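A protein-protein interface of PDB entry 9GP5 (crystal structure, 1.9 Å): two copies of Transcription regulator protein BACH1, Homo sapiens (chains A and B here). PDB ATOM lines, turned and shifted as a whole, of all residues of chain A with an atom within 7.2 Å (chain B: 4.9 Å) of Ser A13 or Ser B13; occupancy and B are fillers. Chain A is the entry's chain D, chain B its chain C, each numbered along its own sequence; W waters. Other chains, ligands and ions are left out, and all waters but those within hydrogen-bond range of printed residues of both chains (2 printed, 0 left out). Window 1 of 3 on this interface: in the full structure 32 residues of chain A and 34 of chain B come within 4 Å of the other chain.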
ATOM      1  N   SER A   9     -20.392 -36.139  27.770  1.00  0.00           N
ATOM      2  CA  SER A   9     -21.678 -36.657  27.349  1.00  0.00           C
ATOM      3  C   SER A   9     -22.053 -36.024  26.012  1.00  0.00           C
ATOM      4  O   SER A   9     -22.173 -34.801  25.887  1.00  0.00           O
ATOM      5  CB  SER A   9     -22.730 -36.454  28.423  1.00  0.00           C
ATOM      6  OG  SER A   9     -24.030 -36.647  27.874  1.00  0.00           O
ATOM      7  N   SER A  10     -22.382 -36.873  25.062  1.00  0.00           N
ATOM      8  CA  SER A  10     -22.847 -36.412  23.775  1.00  0.00           C
ATOM      9  C   SER A  10     -24.337 -36.048  23.802  1.00  0.00           C
ATOM     10  O   SER A  10     -24.780 -35.434  22.847  1.00  0.00           O
ATOM     11  CB  SER A  10     -22.594 -37.460  22.699  1.00  0.00           C
ATOM     12  OG  SER A  10     -23.294 -38.661  23.055  1.00  0.00           O
ATOM     13  N   VAL A  11     -25.123 -36.498  24.788  1.00  0.00           N
ATOM     14  CA  VAL A  11     -26.547 -36.203  24.775  1.00  0.00           C
ATOM     15  C   VAL A  11     -26.957 -35.098  25.767  1.00  0.00           C
ATOM     16  O   VAL A  11     -28.086 -34.635  25.729  1.00  0.00           O
ATOM     17  CB  VAL A  11     -27.375 -37.467  25.033  1.00  0.00           C
ATOM     18  CG1 VAL A  11     -27.043 -38.561  24.007  1.00  0.00           C
ATOM     19  CG2 VAL A  11     -27.222 -37.970  26.449  1.00  0.00           C
ATOM     20  N   HIS A  12     -26.090 -34.720  26.715  1.00  0.00           N
ATOM     21  CA  HIS A  12     -26.429 -33.746  27.728  1.00  0.00           C
ATOM     22  C   HIS A  12     -26.910 -32.409  27.154  1.00  0.00           C
ATOM     23  O   HIS A  12     -27.914 -31.891  27.585  1.00  0.00           O
ATOM     24  CB  HIS A  12     -25.227 -33.468  28.643  1.00  0.00           C
ATOM     25  CG  HIS A  12     -25.555 -32.477  29.710  1.00  0.00           C
ATOM     26  ND1 HIS A  12     -26.373 -32.730  30.794  1.00  0.00           N
ATOM     27  CD2 HIS A  12     -25.035 -31.239  29.923  1.00  0.00           C
ATOM     28  CE1 HIS A  12     -26.480 -31.631  31.531  1.00  0.00           C
ATOM     29  NE2 HIS A  12     -25.652 -30.720  31.066  1.00  0.00           N
ATOM     30  N   SER A  13     -26.228 -31.832  26.179  1.00  0.00           N
ATOM     31  CA  SER A  13     -26.644 -30.515  25.722  1.00  0.00           C
ATOM     32  C   SER A  13     -28.040 -30.578  25.082  1.00  0.00           C
ATOM     33  O   SER A  13     -28.827 -29.668  25.296  1.00  0.00           O
ATOM     34  CB  SER A  13     -25.613 -29.903  24.806  1.00  0.00           C
ATOM     35  OG  SER A  13     -25.561 -30.505  23.503  1.00  0.00           O
ATOM     36  N   THR A  14     -28.322 -31.703  24.403  1.00  0.00           N
ATOM     37  CA  THR A  14     -29.616 -31.951  23.767  1.00  0.00           C
ATOM     38  C   THR A  14     -30.709 -32.112  24.821  1.00  0.00           C
ATOM     39  O   THR A  14     -31.786 -31.528  24.708  1.00  0.00           O
ATOM     40  CB  THR A  14     -29.593 -33.184  22.877  1.00  0.00           C
ATOM     41  OG1 THR A  14     -28.717 -32.816  21.835  1.00  0.00           O
ATOM     42  CG2 THR A  14     -30.957 -33.511  22.295  1.00  0.00           C
ATOM     43  N   ASN A  15     -30.362 -32.790  25.917  1.00  0.00           N
ATOM     44  CA  ASN A  15     -31.293 -32.974  27.007  1.00  0.00           C
ATOM     45  C   ASN A  15     -31.606 -31.659  27.704  1.00  0.00           C
ATOM     46  O   ASN A  15     -32.782 -31.409  28.025  1.00  0.00           O
ATOM     47  CB  ASN A  15     -30.782 -34.017  27.991  1.00  0.00           C
ATOM     48  CG  ASN A  15     -30.786 -35.404  27.392  1.00  0.00           C
ATOM     49  OD1 ASN A  15     -31.383 -35.645  26.341  1.00  0.00           O
ATOM     50  ND2 ASN A  15     -30.045 -36.270  28.043  1.00  0.00           N
ATOM     51  N   VAL A  16     -30.590 -30.825  27.915  1.00  0.00           N
ATOM     52  CA  VAL A  16     -30.832 -29.540  28.526  1.00  0.00           C
ATOM     53  C   VAL A  16     -31.752 -28.699  27.615  1.00  0.00           C
ATOM     54  O   VAL A  16     -32.695 -28.057  28.077  1.00  0.00           O
ATOM     55  CB  VAL A  16     -29.518 -28.816  28.820  1.00  0.00           C
ATOM     56  CG1 VAL A  16     -29.784 -27.374  29.251  1.00  0.00           C
ATOM     57  CG2 VAL A  16     -28.750 -29.525  29.921  1.00  0.00           C
ATOM     58  N   LEU A  17     -31.414 -28.604  26.346  1.00  0.00           N
ATOM     59  CA  LEU A  17     -32.233 -27.795  25.443  1.00  0.00           C
ATOM     60  C   LEU A  17     -33.677 -28.280  25.390  1.00  0.00           C
ATOM     61  O   LEU A  17     -34.581 -27.460  25.395  1.00  0.00           O
ATOM     62  CB  LEU A  17     -31.630 -27.747  24.041  1.00  0.00           C
ATOM     63  CG  LEU A  17     -32.206 -26.654  23.114  1.00  0.00           C
ATOM     64  CD1 LEU A  17     -31.981 -25.258  23.600  1.00  0.00           C
ATOM     65  CD2 LEU A  17     -31.617 -26.793  21.691  1.00  0.00           C
ATOM     66  N   LEU A  18     -33.910 -29.579  25.354  1.00  0.00           N
ATOM     67  CA  LEU A  18     -35.266 -30.086  25.357  1.00  0.00           C
ATOM     68  C   LEU A  18     -36.001 -29.803  26.677  1.00  0.00           C
ATOM     69  O   LEU A  18     -37.221 -29.584  26.650  1.00  0.00           O
ATOM     70  CB  LEU A  18     -35.205 -31.563  24.989  1.00  0.00           C
ATOM     71  CG  LEU A  18     -35.077 -31.818  23.476  1.00  0.00           C
ATOM     72  CD1 LEU A  18     -33.804 -31.236  22.805  1.00  0.00           C
ATOM     73  CD2 LEU A  18     -35.156 -33.294  23.239  1.00  0.00           C
ATOM     74  N   SER A  19     -35.307 -29.797  27.807  1.00  0.00           N
ATOM     75  CA  SER A  19     -35.876 -29.347  29.070  1.00  0.00           C
ATOM     76  C   SER A  19     -36.290 -27.882  29.003  1.00  0.00           C
ATOM     77  O   SER A  19     -37.357 -27.523  29.503  1.00  0.00           O
ATOM     78  CB  SER A  19     -34.896 -29.524  30.242  1.00  0.00           C
ATOM     79  OG  SER A  19     -34.615 -30.900  30.402  1.00  0.00           O
ATOM     80  N   LEU A  20     -35.388 -27.036  28.458  1.00  0.00           N
ATOM     81  CA  LEU A  20     -35.700 -25.624  28.287  1.00  0.00           C
ATOM     82  C   LEU A  20     -36.892 -25.445  27.358  1.00  0.00           C
ATOM     83  O   LEU A  20     -37.719 -24.562  27.585  1.00  0.00           O
ATOM     84  CB  LEU A  20     -34.492 -24.855  27.760  1.00  0.00           C
ATOM     85  CG  LEU A  20     -33.255 -24.826  28.661  1.00  0.00           C
ATOM     86  CD1 LEU A  20     -32.086 -24.155  27.967  1.00  0.00           C
ATOM     87  CD2 LEU A  20     -33.532 -24.111  29.953  1.00  0.00           C
ATOM     88  N   ALA A  87     -34.534 -22.341  17.764  1.00  0.00           N
ATOM     89  CA  ALA A  87     -33.700 -21.915  18.881  1.00  0.00           C
ATOM     90  C   ALA A  87     -33.775 -22.910  20.035  1.00  0.00           C
ATOM     91  O   ALA A  87     -32.746 -23.269  20.643  1.00  0.00           O
ATOM     92  CB  ALA A  87     -34.123 -20.554  19.362  1.00  0.00           C
ATOM     93  N   THR A  89     -35.036 -26.242  19.741  1.00  0.00           N
ATOM     94  CA  THR A  89     -35.058 -27.664  19.409  1.00  0.00           C
ATOM     95  C   THR A  89     -33.969 -28.124  18.443  1.00  0.00           C
ATOM     96  O   THR A  89     -33.838 -29.337  18.225  1.00  0.00           O
ATOM     97  CB  THR A  89     -36.412 -28.073  18.798  1.00  0.00           C
ATOM     98  OG1 THR A  89     -36.611 -27.476  17.499  1.00  0.00           O
ATOM     99  CG2 THR A  89     -37.588 -27.771  19.709  1.00  0.00           C
ATOM    100  N   ALA A  90     -33.242 -27.202  17.776  1.00  0.00           N
ATOM    101  CA  ALA A  90     -32.208 -27.532  16.775  1.00  0.00           C
ATOM    102  C   ALA A  90     -32.806 -28.106  15.491  1.00  0.00           C
ATOM    103  O   ALA A  90     -32.085 -28.603  14.630  1.00  0.00           O
ATOM    104  CB  ALA A  90     -31.126 -28.439  17.349  1.00  0.00           C
ATOM    105  N   ASN A 113     -25.994 -19.941  13.913  1.00  0.00           N
ATOM    106  CA  ASN A 113     -25.979 -21.378  13.619  1.00  0.00           C
ATOM    107  C   ASN A 113     -26.811 -21.682  12.367  1.00  0.00           C
ATOM    108  O   ASN A 113     -27.275 -22.803  12.171  1.00  0.00           O
ATOM    109  CB  ASN A 113     -26.476 -22.228  14.797  1.00  0.00           C
ATOM    110  CG  ASN A 113     -25.680 -22.079  16.082  1.00  0.00           C
ATOM    111  OD1 ASN A 113     -26.247 -22.264  17.157  1.00  0.00           O
ATOM    112  ND2 ASN A 113     -24.400 -21.725  15.993  1.00  0.00           N
ATOM    113  N   VAL B  11     -24.939 -29.375  16.046  1.00  0.00           N
ATOM    114  CA  VAL B  11     -24.117 -28.601  16.951  1.00  0.00           C
ATOM    115  C   VAL B  11     -24.887 -27.517  17.712  1.00  0.00           C
ATOM    116  O   VAL B  11     -24.321 -26.898  18.599  1.00  0.00           O
ATOM    117  CB  VAL B  11     -22.929 -27.972  16.211  1.00  0.00           C
ATOM    118  CG1 VAL B  11     -22.075 -29.055  15.549  1.00  0.00           C
ATOM    119  CG2 VAL B  11     -23.372 -26.907  15.233  1.00  0.00           C
ATOM    120  N   HIS B  12     -26.140 -27.210  17.339  1.00  0.00           N
ATOM    121  CA  HIS B  12     -26.842 -26.070  17.920  1.00  0.00           C
ATOM    122  C   HIS B  12     -27.004 -26.231  19.437  1.00  0.00           C
ATOM    123  O   HIS B  12     -26.778 -25.297  20.178  1.00  0.00           O
ATOM    124  CB  HIS B  12     -28.227 -25.906  17.296  1.00  0.00           C
ATOM    125  CG  HIS B  12     -29.032 -24.839  17.906  1.00  0.00           C
ATOM    126  ND1 HIS B  12     -28.812 -23.478  17.777  1.00  0.00           N
ATOM    127  CD2 HIS B  12     -30.156 -24.973  18.655  1.00  0.00           C
ATOM    128  CE1 HIS B  12     -29.726 -22.840  18.510  1.00  0.00           C
ATOM    129  NE2 HIS B  12     -30.542 -23.720  19.033  1.00  0.00           N
ATOM    130  N   SER B  13     -27.376 -27.402  19.927  1.00  0.00           N
ATOM    131  CA  SER B  13     -27.601 -27.528  21.361  1.00  0.00           C
ATOM    132  C   SER B  13     -26.313 -27.282  22.153  1.00  0.00           C
ATOM    133  O   SER B  13     -26.349 -26.636  23.216  1.00  0.00           O
ATOM    134  CB  SER B  13     -28.274 -28.829  21.673  1.00  0.00           C
ATOM    135  OG  SER B  13     -27.442 -29.968  21.583  1.00  0.00           O
ATOM    136  N   THR B  14     -25.195 -27.740  21.586  1.00  0.00           N
ATOM    137  CA  THR B  14     -23.869 -27.556  22.169  1.00  0.00           C
ATOM    138  C   THR B  14     -23.455 -26.085  22.157  1.00  0.00           C
ATOM    139  O   THR B  14     -22.960 -25.563  23.152  1.00  0.00           O
ATOM    140  CB  THR B  14     -22.819 -28.390  21.439  1.00  0.00           C
ATOM    141  OG1 THR B  14     -23.183 -29.718  21.799  1.00  0.00           O
ATOM    142  CG2 THR B  14     -21.408 -28.104  21.950  1.00  0.00           C
ATOM    143  N   ASN B  15     -23.808 -25.380  21.080  1.00  0.00           N
ATOM    144  CA  ASN B  15     -23.525 -23.962  20.987  1.00  0.00           C
ATOM    145  C   ASN B  15     -24.359 -23.174  21.986  1.00  0.00           C
ATOM    146  O   ASN B  15     -23.842 -22.246  22.639  1.00  0.00           O
ATOM    147  CB  ASN B  15     -23.716 -23.452  19.569  1.00  0.00           C
ATOM    148  CG  ASN B  15     -22.713 -24.063  18.613  1.00  0.00           C
ATOM    149  OD1 ASN B  15     -21.702 -24.644  19.021  1.00  0.00           O
ATOM    150  ND2 ASN B  15     -23.023 -23.928  17.342  1.00  0.00           N
ATOM    151  N   VAL B  16     -25.633 -23.524  22.145  1.00  0.00           N
ATOM    152  CA  VAL B  16     -26.441 -22.839  23.126  1.00  0.00           C
ATOM    153  C   VAL B  16     -25.856 -23.063  24.538  1.00  0.00           C
ATOM    154  O   VAL B  16     -25.712 -22.134  25.341  1.00  0.00           O
ATOM    155  CB  VAL B  16     -27.894 -23.307  23.068  1.00  0.00           C
ATOM    156  CG1 VAL B  16     -28.693 -22.756  24.240  1.00  0.00           C
ATOM    157  CG2 VAL B  16     -28.539 -22.878  21.766  1.00  0.00           C
ATOM    158  N   LEU B  17     -25.595 -24.303  24.885  1.00  0.00           N
ATOM    159  CA  LEU B  17     -25.066 -24.569  26.221  1.00  0.00           C
ATOM    160  C   LEU B  17     -23.765 -23.838  26.458  1.00  0.00           C
ATOM    161  O   LEU B  17     -23.568 -23.318  27.554  1.00  0.00           O
ATOM    162  CB  LEU B  17     -24.900 -26.074  26.461  1.00  0.00           C
ATOM    163  CG  LEU B  17     -24.684 -26.500  27.927  1.00  0.00           C
ATOM    164  CD1 LEU B  17     -25.851 -26.168  28.808  1.00  0.00           C
ATOM    165  CD2 LEU B  17     -24.426 -27.987  28.045  1.00  0.00           C
ATOM    166  N   ALA B  90     -21.240 -30.349  29.664  1.00  0.00           N
ATOM    167  CA  ALA B  90     -21.330 -31.753  29.258  1.00  0.00           C
ATOM    168  C   ALA B  90     -20.022 -32.504  29.460  1.00  0.00           C
ATOM    169  O   ALA B  90     -19.887 -33.634  29.002  1.00  0.00           O
ATOM    170  CB  ALA B  90     -21.835 -31.879  27.829  1.00  0.00           C
HETATM  171  O   HOH W   1     -22.326 -30.823  24.237  1.00  0.00           O
HETATM  172  O   HOH W   2     -29.908 -31.159  19.638  1.00  0.00           O
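O of Ala A87 sits at hydrogen-bond distance from NE2 of His B12 (2.8 Å).
OD1 of Asn A113 sits at hydrogen-bond distance from ND1 of His B12, at 2.9 Å.
The side-chain hydroxyl (OG) of Ser B13 lies within hydrogen-bond range of the side-chain hydroxyl (OG) of Ser A13 (2.7 Å).
The side-chain hydroxyl (OG1) of Thr A14 is in hydrogen-bond range of the side-chain hydroxyl (OG) of Ser B13.
OG1 of Thr B14 lies within hydrogen-bond range of OG of Ser A13, at 3.0 Å.
ND2 of Asn A113 lies close to ND2 of Asn B15 (2.9 Å).
The backbone carbonyl oxygen of Ala B90 lies within hydrogen-bond range of the backbone NH of Ser A9, at 2.8 Å.
O of Val B11 sits close to ND2 of Asn B15 (3.5 Å).
The backbone NH (N) of Val A11 is in hydrogen-bond range of the side-chain hydroxyl (OG) of Ser A9 (3.3 Å).
The side-chain hydroxyl of Ser A9 lies within hydrogen-bond range of the backbone NH of His A12 (3.0 Å).
Among the printed residues, merely in contact across the chains: Ala A90 with His B12, His A12 with Ala B90, His A12 with Leu B17, Leu A17 with His B12, Leu A17 with Ser B13 and Ser A13 with Leu B17.
Of the printed residues of chain B, Ser A9 touches Ala B90.
Ser A13 touches just these residues of chain B: Ser B13, Thr B14 and Leu B17.
Of the printed residues of chain B, Ala A87 touches His B12 (2.8 Å).
Ser B13 touches three residues of chain A.
Printed residues of chain A within 4 Å of Thr B14: Ser A13.
Of the 8 printed residues of chain B, 6 touch a printed residue of chain A.
His A12 touches Leu B17, and with the chains exchanged Leu A17 touches His B12.
His A12 touches Ala B90, and with the chains exchanged Ala A90 touches His B12.
Ser A13 touches Thr B14, and with the chains exchanged Thr A14 touches Ser B13.
Ser A13 touches Leu B17, and with the chains exchanged Leu A17 touches Ser B13.
Water W1 lies within hydrogen-bond range of OG1 of Thr B14 (2.8 Å) and OG of Ser A13 (3.3 Å).
Water W2 lies within hydrogen-bond range of the side-chain hydroxyl of Thr A14 and the side-chain hydroxyl of Ser B13.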
